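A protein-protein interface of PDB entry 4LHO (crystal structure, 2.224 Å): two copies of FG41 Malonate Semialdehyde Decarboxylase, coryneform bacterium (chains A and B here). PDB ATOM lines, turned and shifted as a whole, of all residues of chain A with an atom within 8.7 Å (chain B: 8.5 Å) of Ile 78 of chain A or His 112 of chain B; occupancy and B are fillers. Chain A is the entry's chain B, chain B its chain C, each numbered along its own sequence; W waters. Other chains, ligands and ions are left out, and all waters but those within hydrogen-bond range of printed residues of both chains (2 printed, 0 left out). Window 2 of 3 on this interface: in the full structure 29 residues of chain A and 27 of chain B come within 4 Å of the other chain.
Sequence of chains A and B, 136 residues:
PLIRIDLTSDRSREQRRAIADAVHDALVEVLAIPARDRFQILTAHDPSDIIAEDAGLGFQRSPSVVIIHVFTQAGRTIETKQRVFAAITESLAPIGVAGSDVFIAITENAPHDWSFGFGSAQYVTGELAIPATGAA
The side-chain amino group (NZ) of Lys 81 of chain A lies within salt-bridge range of the side-chain carboxylate (OD2) of Asp 113 of chain B.
The backbone NH (N) of Ile 104 of chain A lies within hydrogen-bond range of the backbone carbonyl oxygen (O) of Ser 115 of chain B, 2.8 Å away.
O of Ile 106 of chain A sits at hydrogen-bond distance from ND2 of Asn 109 of chain B, at 2.9 Å.
O of Asp 113 of chain B lies within hydrogen-bond range of N of Ile 106 of chain A, 2.9 Å away.
The side-chain carboxylate (OE2) of Glu 108 of chain A lies within salt-bridge range of the side-chain amino group (NZ) of Lys 81 of chain A, at 2.7 Å.
The side-chain amide oxygen (OD1) of Asn 109 of chain B lies within hydrogen-bond range of the indole nitrogen (NE1) of Trp 114 of chain B (2.8 Å).
The side-chain carboxylate (OD1) of Asp 113 of chain B is in hydrogen-bond range of the backbone NH (N) of Ala 110 of chain B (2.9 Å).
The indole nitrogen (NE1) of Trp 114 of chain B lies close to the backbone carbonyl oxygen (O) of Ala 110 of chain B (3.3 Å).
The backbone carbonyl oxygen of Ser 120 of chain B sits at hydrogen-bond distance from the side-chain hydroxyl of Ser 115 of chain B (2.6 Å).
Among the printed residues, pairs that only touch across the chains: Ile 78 of chain A with His 112 of chain B (3.6 Å), Lys 81 of chain A with His 112 of chain B (3.6 Å), Gln 82 of chain A with Val 124 of chain B (3.3 Å), Phe 85 of chain A with His 112 of chain B (3.8 Å), Phe 85 of chain A with Asp 113 of chain B (3.8 Å), Phe 85 of chain A with Trp 114 of chain B (3.7 Å), Phe 85 of chain A with Ser 115 of chain B (3.8 Å), Phe 85 of chain A with Ala 121 of chain B (3.9 Å), Ile 104 of chain A with Asp 113 of chain B (3.98 Å), Ile 104 of chain A with Trp 114 of chain B (3.6 Å), Ala 105 of chain A with Asp 113 of chain B (3.4 Å) and Ala 105 of chain A with Trp 114 of chain B (3.7 Å).
Of chain B, only His 112 (3.6 Å) comes within 4 Å of Ile 78 of chain A.
Printed residues of chain B within 4 Å of Ile 104 of chain A: Asp 113, Trp 114 and Ser 115.
Printed residues of chain B within 4 Å of Ala 105 of chain A: Asp 113 (3.4 Å) and Trp 114 (3.7 Å).
No residue of chain A comes within 4 Å of Pro 111 of chain B.
His 112 of chain B touches three residues of chain A.
Of the printed residues of chain A, Asp 113 of chain B touches Lys 81, Phe 85, Ile 104, Ala 105 and Ile 106.
The nearest residue of chain A that does not touch His 112 of chain B is Ile 106 of chain A (5.1 Å).
Among the printed residues, Asp or Glu carboxylates within 4 Å of a Lys or Arg side-chain nitrogen of the other chain: Lys 81 of chain A with Asp 113 of chain B (2.7 Å).
No position is printed for both chains.
Water W1 lies within hydrogen-bond range of O of Arg 76 of chain A (2.5 Å), NZ of Lys 81 of chain A (3.0 Å), N of Ile 78 of chain A (3.3 Å) and NE2 of His 112 of chain B (3.4 Å).
Water W2 bridges the backbone NH of Ala 121 of chain B (3.0 Å) and the side-chain amide nitrogen of Gln 82 of chain A (3.1 Å).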
ATOM      1  N   GLY A  75      37.855  -1.673  -7.103  1.00  0.00           N
ATOM      2  CA  GLY A  75      38.337  -2.877  -6.457  1.00  0.00           C
ATOM      3  C   GLY A  75      37.245  -3.751  -5.865  1.00  0.00           C
ATOM      4  O   GLY A  75      37.416  -4.963  -5.766  1.00  0.00           O
ATOM      5  N   ARG A  76      36.120  -3.166  -5.469  1.00  0.00           N
ATOM      6  CA  ARG A  76      35.094  -3.977  -4.825  1.00  0.00           C
ATOM      7  C   ARG A  76      34.279  -4.733  -5.868  1.00  0.00           C
ATOM      8  O   ARG A  76      33.996  -4.242  -6.962  1.00  0.00           O
ATOM      9  CB  ARG A  76      34.235  -3.125  -3.911  1.00  0.00           C
ATOM     10  CG  ARG A  76      35.063  -2.201  -2.988  1.00  0.00           C
ATOM     11  CD  ARG A  76      35.672  -2.918  -1.795  1.00  0.00           C
ATOM     12  NE  ARG A  76      36.185  -1.981  -0.793  1.00  0.00           N
ATOM     13  CZ  ARG A  76      36.588  -2.331   0.432  1.00  0.00           C
ATOM     14  NH1 ARG A  76      36.530  -3.594   0.813  1.00  0.00           N
ATOM     15  NH2 ARG A  76      37.033  -1.419   1.286  1.00  0.00           N
ATOM     16  N   THR A  77      33.951  -5.976  -5.557  1.00  0.00           N
ATOM     17  CA  THR A  77      33.204  -6.804  -6.491  1.00  0.00           C
ATOM     18  C   THR A  77      31.734  -6.398  -6.563  1.00  0.00           C
ATOM     19  O   THR A  77      31.202  -5.702  -5.687  1.00  0.00           O
ATOM     20  CB  THR A  77      33.224  -8.269  -6.049  1.00  0.00           C
ATOM     21  OG1 THR A  77      32.589  -8.379  -4.770  1.00  0.00           O
ATOM     22  CG2 THR A  77      34.663  -8.779  -5.940  1.00  0.00           C
ATOM     23  N   ILE A  78      31.078  -6.877  -7.607  1.00  0.00           N
ATOM     24  CA  ILE A  78      29.652  -6.737  -7.728  1.00  0.00           C
ATOM     25  C   ILE A  78      28.934  -7.193  -6.461  1.00  0.00           C
ATOM     26  O   ILE A  78      28.080  -6.478  -5.932  1.00  0.00           O
ATOM     27  CB  ILE A  78      29.169  -7.521  -8.917  1.00  0.00           C
ATOM     28  CG1 ILE A  78      29.751  -6.878 -10.177  1.00  0.00           C
ATOM     29  CG2 ILE A  78      27.641  -7.563  -8.909  1.00  0.00           C
ATOM     30  CD1 ILE A  78      29.281  -7.483 -11.527  1.00  0.00           C
ATOM     31  N   GLU A  79      29.305  -8.364  -5.953  1.00  0.00           N
ATOM     32  CA  GLU A  79      28.599  -8.961  -4.828  1.00  0.00           C
ATOM     33  C   GLU A  79      28.832  -8.153  -3.570  1.00  0.00           C
ATOM     34  O   GLU A  79      27.928  -7.952  -2.752  1.00  0.00           O
ATOM     35  CB  GLU A  79      29.043 -10.410  -4.619  1.00  0.00           C
ATOM     36  N   THR A  80      30.045  -7.663  -3.396  1.00  0.00           N
ATOM     37  CA  THR A  80      30.321  -6.779  -2.268  1.00  0.00           C
ATOM     38  C   THR A  80      29.436  -5.526  -2.356  1.00  0.00           C
ATOM     39  O   THR A  80      28.933  -5.025  -1.340  1.00  0.00           O
ATOM     40  CB  THR A  80      31.790  -6.396  -2.242  1.00  0.00           C
ATOM     41  OG1 THR A  80      32.574  -7.583  -2.079  1.00  0.00           O
ATOM     42  CG2 THR A  80      32.099  -5.433  -1.097  1.00  0.00           C
ATOM     43  N   LYS A  81      29.206  -5.044  -3.576  1.00  0.00           N
ATOM     44  CA  LYS A  81      28.371  -3.860  -3.753  1.00  0.00           C
ATOM     45  C   LYS A  81      26.923  -4.180  -3.390  1.00  0.00           C
ATOM     46  O   LYS A  81      26.289  -3.394  -2.689  1.00  0.00           O
ATOM     47  CB  LYS A  81      28.516  -3.299  -5.173  1.00  0.00           C
ATOM     48  CG  LYS A  81      29.870  -2.574  -5.397  1.00  0.00           C
ATOM     49  CD  LYS A  81      30.123  -2.261  -6.886  1.00  0.00           C
ATOM     50  CE  LYS A  81      31.463  -1.533  -7.072  1.00  0.00           C
ATOM     51  NZ  LYS A  81      31.708  -1.169  -8.491  1.00  0.00           N
ATOM     52  N   GLN A  82      26.418  -5.338  -3.824  1.00  0.00           N
ATOM     53  CA  GLN A  82      25.046  -5.741  -3.472  1.00  0.00           C
ATOM     54  C   GLN A  82      24.884  -5.767  -1.961  1.00  0.00           C
ATOM     55  O   GLN A  82      23.875  -5.324  -1.404  1.00  0.00           O
ATOM     56  CB  GLN A  82      24.712  -7.087  -4.048  1.00  0.00           C
ATOM     57  CG  GLN A  82      24.501  -7.056  -5.524  1.00  0.00           C
ATOM     58  CD  GLN A  82      24.214  -8.425  -6.114  1.00  0.00           C
ATOM     59  OE1 GLN A  82      25.117  -9.242  -6.253  1.00  0.00           O
ATOM     60  NE2 GLN A  82      22.961  -8.676  -6.483  1.00  0.00           N
ATOM     61  N   ARG A  83      25.925  -6.197  -1.283  1.00  0.00           N
ATOM     62  CA  ARG A  83      25.872  -6.282   0.172  1.00  0.00           C
ATOM     63  C   ARG A  83      25.917  -4.919   0.820  1.00  0.00           C
ATOM     64  O   ARG A  83      25.321  -4.702   1.875  1.00  0.00           O
ATOM     65  CB  ARG A  83      27.051  -7.117   0.679  1.00  0.00           C
ATOM     66  CG  ARG A  83      27.060  -8.564   0.183  1.00  0.00           C
ATOM     67  CD  ARG A  83      27.854  -9.483   1.145  1.00  0.00           C
ATOM     68  NE  ARG A  83      27.218  -9.480   2.476  1.00  0.00           N
ATOM     69  CZ  ARG A  83      27.832  -9.270   3.650  1.00  0.00           C
ATOM     70  NH1 ARG A  83      29.153  -9.047   3.721  1.00  0.00           N
ATOM     71  NH2 ARG A  83      27.101  -9.289   4.769  1.00  0.00           N
ATOM     72  N   VAL A  84      26.666  -3.998   0.208  1.00  0.00           N
ATOM     73  CA  VAL A  84      26.680  -2.602   0.667  1.00  0.00           C
ATOM     74  C   VAL A  84      25.254  -2.026   0.642  1.00  0.00           C
ATOM     75  O   VAL A  84      24.772  -1.499   1.636  1.00  0.00           O
ATOM     76  CB  VAL A  84      27.654  -1.716  -0.192  1.00  0.00           C
ATOM     77  CG1 VAL A  84      27.404  -0.221   0.049  1.00  0.00           C
ATOM     78  CG2 VAL A  84      29.101  -2.055   0.142  1.00  0.00           C
ATOM     79  N   PHE A  85      24.593  -2.157  -0.498  1.00  0.00           N
ATOM     80  CA  PHE A  85      23.237  -1.656  -0.681  1.00  0.00           C
ATOM     81  C   PHE A  85      22.299  -2.263   0.362  1.00  0.00           C
ATOM     82  O   PHE A  85      21.501  -1.557   1.012  1.00  0.00           O
ATOM     83  CB  PHE A  85      22.755  -2.048  -2.063  1.00  0.00           C
ATOM     84  CG  PHE A  85      23.534  -1.439  -3.191  1.00  0.00           C
ATOM     85  CD1 PHE A  85      24.186  -0.229  -3.045  1.00  0.00           C
ATOM     86  CD2 PHE A  85      23.580  -2.060  -4.409  1.00  0.00           C
ATOM     87  CE1 PHE A  85      24.862   0.333  -4.090  1.00  0.00           C
ATOM     88  CE2 PHE A  85      24.273  -1.494  -5.467  1.00  0.00           C
ATOM     89  CZ  PHE A  85      24.903  -0.289  -5.294  1.00  0.00           C
ATOM     90  N   ILE A 104      20.645   4.591  -3.912  1.00  0.00           N
ATOM     91  CA  ILE A 104      22.087   4.528  -3.665  1.00  0.00           C
ATOM     92  C   ILE A 104      22.849   4.475  -4.973  1.00  0.00           C
ATOM     93  O   ILE A 104      22.444   3.782  -5.926  1.00  0.00           O
ATOM     94  CB  ILE A 104      22.481   3.335  -2.786  1.00  0.00           C
ATOM     95  CG1 ILE A 104      21.551   3.235  -1.589  1.00  0.00           C
ATOM     96  CG2 ILE A 104      23.958   3.444  -2.313  1.00  0.00           C
ATOM     97  CD1 ILE A 104      21.828   2.028  -0.699  1.00  0.00           C
ATOM     98  N   ALA A 105      23.930   5.255  -5.048  1.00  0.00           N
ATOM     99  CA  ALA A 105      24.797   5.233  -6.239  1.00  0.00           C
ATOM    100  C   ALA A 105      26.267   5.138  -5.845  1.00  0.00           C
ATOM    101  O   ALA A 105      26.660   5.678  -4.830  1.00  0.00           O
ATOM    102  CB  ALA A 105      24.579   6.450  -7.089  1.00  0.00           C
ATOM    103  N   ILE A 106      27.061   4.467  -6.674  1.00  0.00           N
ATOM    104  CA  ILE A 106      28.499   4.348  -6.443  1.00  0.00           C
ATOM    105  C   ILE A 106      29.295   4.918  -7.620  1.00  0.00           C
ATOM    106  O   ILE A 106      29.015   4.614  -8.774  1.00  0.00           O
ATOM    107  CB  ILE A 106      28.936   2.852  -6.242  1.00  0.00           C
ATOM    108  CG1 ILE A 106      28.249   2.262  -5.009  1.00  0.00           C
ATOM    109  CG2 ILE A 106      30.433   2.767  -6.123  1.00  0.00           C
ATOM    110  CD1 ILE A 106      28.502   0.788  -4.804  1.00  0.00           C
ATOM    111  N   GLU A 108      33.389   5.550  -8.813  1.00  0.00           N
ATOM    112  CA  GLU A 108      34.712   5.053  -8.486  1.00  0.00           C
ATOM    113  C   GLU A 108      35.864   5.948  -8.956  1.00  0.00           C
ATOM    114  O   GLU A 108      35.759   6.669  -9.943  1.00  0.00           O
ATOM    115  CB  GLU A 108      34.884   3.655  -9.070  1.00  0.00           C
ATOM    116  CG  GLU A 108      34.227   2.578  -8.234  1.00  0.00           C
ATOM    117  CD  GLU A 108      34.378   1.196  -8.848  1.00  0.00           C
ATOM    118  OE1 GLU A 108      34.854   1.112 -10.011  1.00  0.00           O
ATOM    119  OE2 GLU A 108      34.036   0.209  -8.153  1.00  0.00           O
ATOM    120  N   GLN B  73      25.282   5.450 -16.240  1.00  0.00           N
ATOM    121  CA  GLN B  73      26.100   4.277 -16.507  1.00  0.00           C
ATOM    122  C   GLN B  73      26.755   4.440 -17.868  1.00  0.00           C
ATOM    123  O   GLN B  73      26.214   5.122 -18.741  1.00  0.00           O
ATOM    124  CB  GLN B  73      25.271   2.992 -16.427  1.00  0.00           C
ATOM    125  CG  GLN B  73      24.234   2.885 -17.485  1.00  0.00           C
ATOM    126  CD  GLN B  73      23.259   1.763 -17.223  1.00  0.00           C
ATOM    127  OE1 GLN B  73      22.957   0.965 -18.122  1.00  0.00           O
ATOM    128  NE2 GLN B  73      22.730   1.706 -16.005  1.00  0.00           N
ATOM    129  N   ASN B 109      29.468   5.471 -14.444  1.00  0.00           N
ATOM    130  CA  ASN B 109      29.725   4.275 -13.683  1.00  0.00           C
ATOM    131  C   ASN B 109      29.137   3.073 -14.414  1.00  0.00           C
ATOM    132  O   ASN B 109      28.832   3.175 -15.606  1.00  0.00           O
ATOM    133  CB  ASN B 109      29.192   4.417 -12.262  1.00  0.00           C
ATOM    134  CG  ASN B 109      27.682   4.659 -12.205  1.00  0.00           C
ATOM    135  OD1 ASN B 109      26.933   4.493 -13.182  1.00  0.00           O
ATOM    136  ND2 ASN B 109      27.235   5.012 -11.027  1.00  0.00           N
ATOM    137  N   ALA B 110      28.963   1.953 -13.709  1.00  0.00           N
ATOM    138  CA  ALA B 110      28.358   0.750 -14.302  1.00  0.00           C
ATOM    139  C   ALA B 110      26.948   0.459 -13.726  1.00  0.00           C
ATOM    140  O   ALA B 110      26.550   1.051 -12.713  1.00  0.00           O
ATOM    141  CB  ALA B 110      29.280  -0.449 -14.088  1.00  0.00           C
ATOM    142  N   PRO B 111      26.201  -0.453 -14.364  1.00  0.00           N
ATOM    143  CA  PRO B 111      24.851  -0.812 -13.903  1.00  0.00           C
ATOM    144  C   PRO B 111      24.835  -1.415 -12.509  1.00  0.00           C
ATOM    145  O   PRO B 111      23.856  -1.240 -11.746  1.00  0.00           O
ATOM    146  CB  PRO B 111      24.383  -1.836 -14.940  1.00  0.00           C
ATOM    147  CG  PRO B 111      25.171  -1.509 -16.175  1.00  0.00           C
ATOM    148  CD  PRO B 111      26.509  -1.061 -15.674  1.00  0.00           C
ATOM    149  N   HIS B 112      25.912  -2.099 -12.155  1.00  0.00           N
ATOM    150  CA  HIS B 112      25.979  -2.691 -10.825  1.00  0.00           C
ATOM    151  C   HIS B 112      26.277  -1.648  -9.734  1.00  0.00           C
ATOM    152  O   HIS B 112      26.373  -1.975  -8.551  1.00  0.00           O
ATOM    153  CB  HIS B 112      26.977  -3.881 -10.790  1.00  0.00           C
ATOM    154  CG  HIS B 112      28.370  -3.551 -11.228  1.00  0.00           C
ATOM    155  ND1 HIS B 112      28.906  -3.991 -12.422  1.00  0.00           N
ATOM    156  CD2 HIS B 112      29.355  -2.855 -10.609  1.00  0.00           C
ATOM    157  CE1 HIS B 112      30.154  -3.569 -12.524  1.00  0.00           C
ATOM    158  NE2 HIS B 112      30.450  -2.878 -11.436  1.00  0.00           N
ATOM    159  N   ASP B 113      26.414  -0.378 -10.126  1.00  0.00           N
ATOM    160  CA  ASP B 113      26.706   0.674  -9.154  1.00  0.00           C
ATOM    161  C   ASP B 113      25.434   1.413  -8.674  1.00  0.00           C
ATOM    162  O   ASP B 113      25.517   2.513  -8.109  1.00  0.00           O
ATOM    163  CB  ASP B 113      27.716   1.657  -9.741  1.00  0.00           C
ATOM    164  CG  ASP B 113      29.101   1.044  -9.904  1.00  0.00           C
ATOM    165  OD1 ASP B 113      29.741   1.298 -10.945  1.00  0.00           O
ATOM    166  OD2 ASP B 113      29.539   0.309  -8.999  1.00  0.00           O
ATOM    167  N   TRP B 114      24.268   0.800  -8.898  1.00  0.00           N
ATOM    168  CA  TRP B 114      22.975   1.446  -8.626  1.00  0.00           C
ATOM    169  C   TRP B 114      22.030   0.628  -7.746  1.00  0.00           C
ATOM    170  O   TRP B 114      21.794  -0.557  -7.999  1.00  0.00           O
ATOM    171  CB  TRP B 114      22.243   1.781  -9.943  1.00  0.00           C
ATOM    172  CG  TRP B 114      23.016   2.715 -10.810  1.00  0.00           C
ATOM    173  CD1 TRP B 114      23.882   2.378 -11.795  1.00  0.00           C
ATOM    174  CD2 TRP B 114      23.016   4.146 -10.749  1.00  0.00           C
ATOM    175  NE1 TRP B 114      24.441   3.504 -12.347  1.00  0.00           N
ATOM    176  CE2 TRP B 114      23.916   4.605 -11.730  1.00  0.00           C
ATOM    177  CE3 TRP B 114      22.359   5.077  -9.953  1.00  0.00           C
ATOM    178  CZ2 TRP B 114      24.157   5.971 -11.953  1.00  0.00           C
ATOM    179  CZ3 TRP B 114      22.594   6.427 -10.174  1.00  0.00           C
ATOM    180  CH2 TRP B 114      23.485   6.860 -11.166  1.00  0.00           C
ATOM    181  N   SER B 115      21.466   1.279  -6.737  1.00  0.00           N
ATOM    182  CA  SER B 115      20.292   0.764  -6.053  1.00  0.00           C
ATOM    183  C   SER B 115      19.118   1.755  -6.099  1.00  0.00           C
ATOM    184  O   SER B 115      19.185   2.818  -5.488  1.00  0.00           O
ATOM    185  CB  SER B 115      20.611   0.450  -4.598  1.00  0.00           C
ATOM    186  OG  SER B 115      19.468  -0.160  -3.987  1.00  0.00           O
ATOM    187  N   PHE B 116      18.031   1.378  -6.773  1.00  0.00           N
ATOM    188  CA  PHE B 116      16.865   2.238  -6.923  1.00  0.00           C
ATOM    189  C   PHE B 116      15.891   2.133  -5.760  1.00  0.00           C
ATOM    190  O   PHE B 116      14.911   2.855  -5.710  1.00  0.00           O
ATOM    191  CB  PHE B 116      16.121   1.946  -8.217  1.00  0.00           C
ATOM    192  CG  PHE B 116      16.934   2.200  -9.446  1.00  0.00           C
ATOM    193  CD1 PHE B 116      16.694   3.295 -10.236  1.00  0.00           C
ATOM    194  CD2 PHE B 116      17.956   1.346  -9.806  1.00  0.00           C
ATOM    195  CE1 PHE B 116      17.449   3.546 -11.369  1.00  0.00           C
ATOM    196  CE2 PHE B 116      18.707   1.592 -10.947  1.00  0.00           C
ATOM    197  CZ  PHE B 116      18.442   2.704 -11.727  1.00  0.00           C
ATOM    198  N   SER B 120      18.219  -3.201  -2.972  1.00  0.00           N
ATOM    199  CA  SER B 120      18.482  -4.117  -4.071  1.00  0.00           C
ATOM    200  C   SER B 120      19.187  -3.409  -5.261  1.00  0.00           C
ATOM    201  O   SER B 120      18.987  -2.217  -5.530  1.00  0.00           O
ATOM    202  CB  SER B 120      17.148  -4.739  -4.507  1.00  0.00           C
ATOM    203  OG  SER B 120      17.277  -5.630  -5.601  1.00  0.00           O
ATOM    204  N   ALA B 121      20.014  -4.158  -5.968  1.00  0.00           N
ATOM    205  CA  ALA B 121      20.643  -3.685  -7.186  1.00  0.00           C
ATOM    206  C   ALA B 121      19.872  -4.172  -8.387  1.00  0.00           C
ATOM    207  O   ALA B 121      20.212  -5.188  -8.975  1.00  0.00           O
ATOM    208  CB  ALA B 121      22.098  -4.196  -7.254  1.00  0.00           C
ATOM    209  N   GLN B 122      18.874  -3.414  -8.803  1.00  0.00           N
ATOM    210  CA  GLN B 122      17.886  -3.903  -9.746  1.00  0.00           C
ATOM    211  C   GLN B 122      18.464  -4.333 -11.089  1.00  0.00           C
ATOM    212  O   GLN B 122      17.877  -5.215 -11.734  1.00  0.00           O
ATOM    213  CB  GLN B 122      16.751  -2.883  -9.967  1.00  0.00           C
ATOM    214  CG  GLN B 122      15.778  -2.675  -8.778  1.00  0.00           C
ATOM    215  CD  GLN B 122      16.414  -1.842  -7.658  1.00  0.00           C
ATOM    216  OE1 GLN B 122      17.478  -1.259  -7.840  1.00  0.00           O
ATOM    217  NE2 GLN B 122      15.786  -1.822  -6.495  1.00  0.00           N
ATOM    218  N   TYR B 123      19.561  -3.703 -11.543  1.00  0.00           N
ATOM    219  CA  TYR B 123      20.141  -4.088 -12.824  1.00  0.00           C
ATOM    220  C   TYR B 123      20.868  -5.431 -12.658  1.00  0.00           C
ATOM    221  O   TYR B 123      20.922  -6.215 -13.589  1.00  0.00           O
ATOM    222  CB  TYR B 123      21.144  -3.060 -13.371  1.00  0.00           C
ATOM    223  CG  TYR B 123      20.554  -1.777 -13.883  1.00  0.00           C
ATOM    224  CD1 TYR B 123      19.558  -1.755 -14.855  1.00  0.00           C
ATOM    225  CD2 TYR B 123      20.976  -0.575 -13.352  1.00  0.00           C
ATOM    226  CE1 TYR B 123      19.019  -0.553 -15.295  1.00  0.00           C
ATOM    227  CE2 TYR B 123      20.459   0.613 -13.773  1.00  0.00           C
ATOM    228  CZ  TYR B 123      19.485   0.637 -14.741  1.00  0.00           C
ATOM    229  OH  TYR B 123      19.024   1.878 -15.113  1.00  0.00           O
ATOM    230  N   VAL B 124      21.461  -5.662 -11.489  1.00  0.00           N
ATOM    231  CA  VAL B 124      22.198  -6.870 -11.256  1.00  0.00           C
ATOM    232  C   VAL B 124      21.227  -8.063 -11.126  1.00  0.00           C
ATOM    233  O   VAL B 124      21.456  -9.093 -11.714  1.00  0.00           O
ATOM    234  CB  VAL B 124      23.035  -6.751  -9.998  1.00  0.00           C
ATOM    235  CG1 VAL B 124      23.715  -8.087  -9.690  1.00  0.00           C
ATOM    236  CG2 VAL B 124      24.071  -5.635 -10.158  1.00  0.00           C
ATOM    237  N   THR B 125      20.136  -7.899 -10.380  1.00  0.00           N
ATOM    238  CA  THR B 125      19.198  -8.984 -10.139  1.00  0.00           C
ATOM    239  C   THR B 125      18.367  -9.332 -11.357  1.00  0.00           C
ATOM    240  O   THR B 125      17.803 -10.419 -11.398  1.00  0.00           O
ATOM    241  CB  THR B 125      18.195  -8.650  -9.004  1.00  0.00           C
ATOM    242  OG1 THR B 125      17.346  -7.564  -9.406  1.00  0.00           O
ATOM    243  CG2 THR B 125      18.914  -8.307  -7.750  1.00  0.00           C
ATOM    244  N   ILE B 130      18.907  -3.517 -18.526  1.00  0.00           N
ATOM    245  CA  ILE B 130      20.030  -2.643 -18.837  1.00  0.00           C
ATOM    246  C   ILE B 130      19.984  -2.199 -20.298  1.00  0.00           C
ATOM    247  O   ILE B 130      20.169  -3.021 -21.197  1.00  0.00           O
ATOM    248  CB  ILE B 130      21.369  -3.393 -18.634  1.00  0.00           C
ATOM    249  CG1 ILE B 130      21.437  -3.984 -17.229  1.00  0.00           C
ATOM    250  CG2 ILE B 130      22.544  -2.441 -18.904  1.00  0.00           C
ATOM    251  CD1 ILE B 130      22.713  -4.800 -16.928  1.00  0.00           C
HETATM  252  O   HOH W   1      32.339  -4.078  -8.877  1.00  0.00           O
HETATM  253  O   HOH W   2      21.002  -6.788  -4.993  1.00  0.00           O
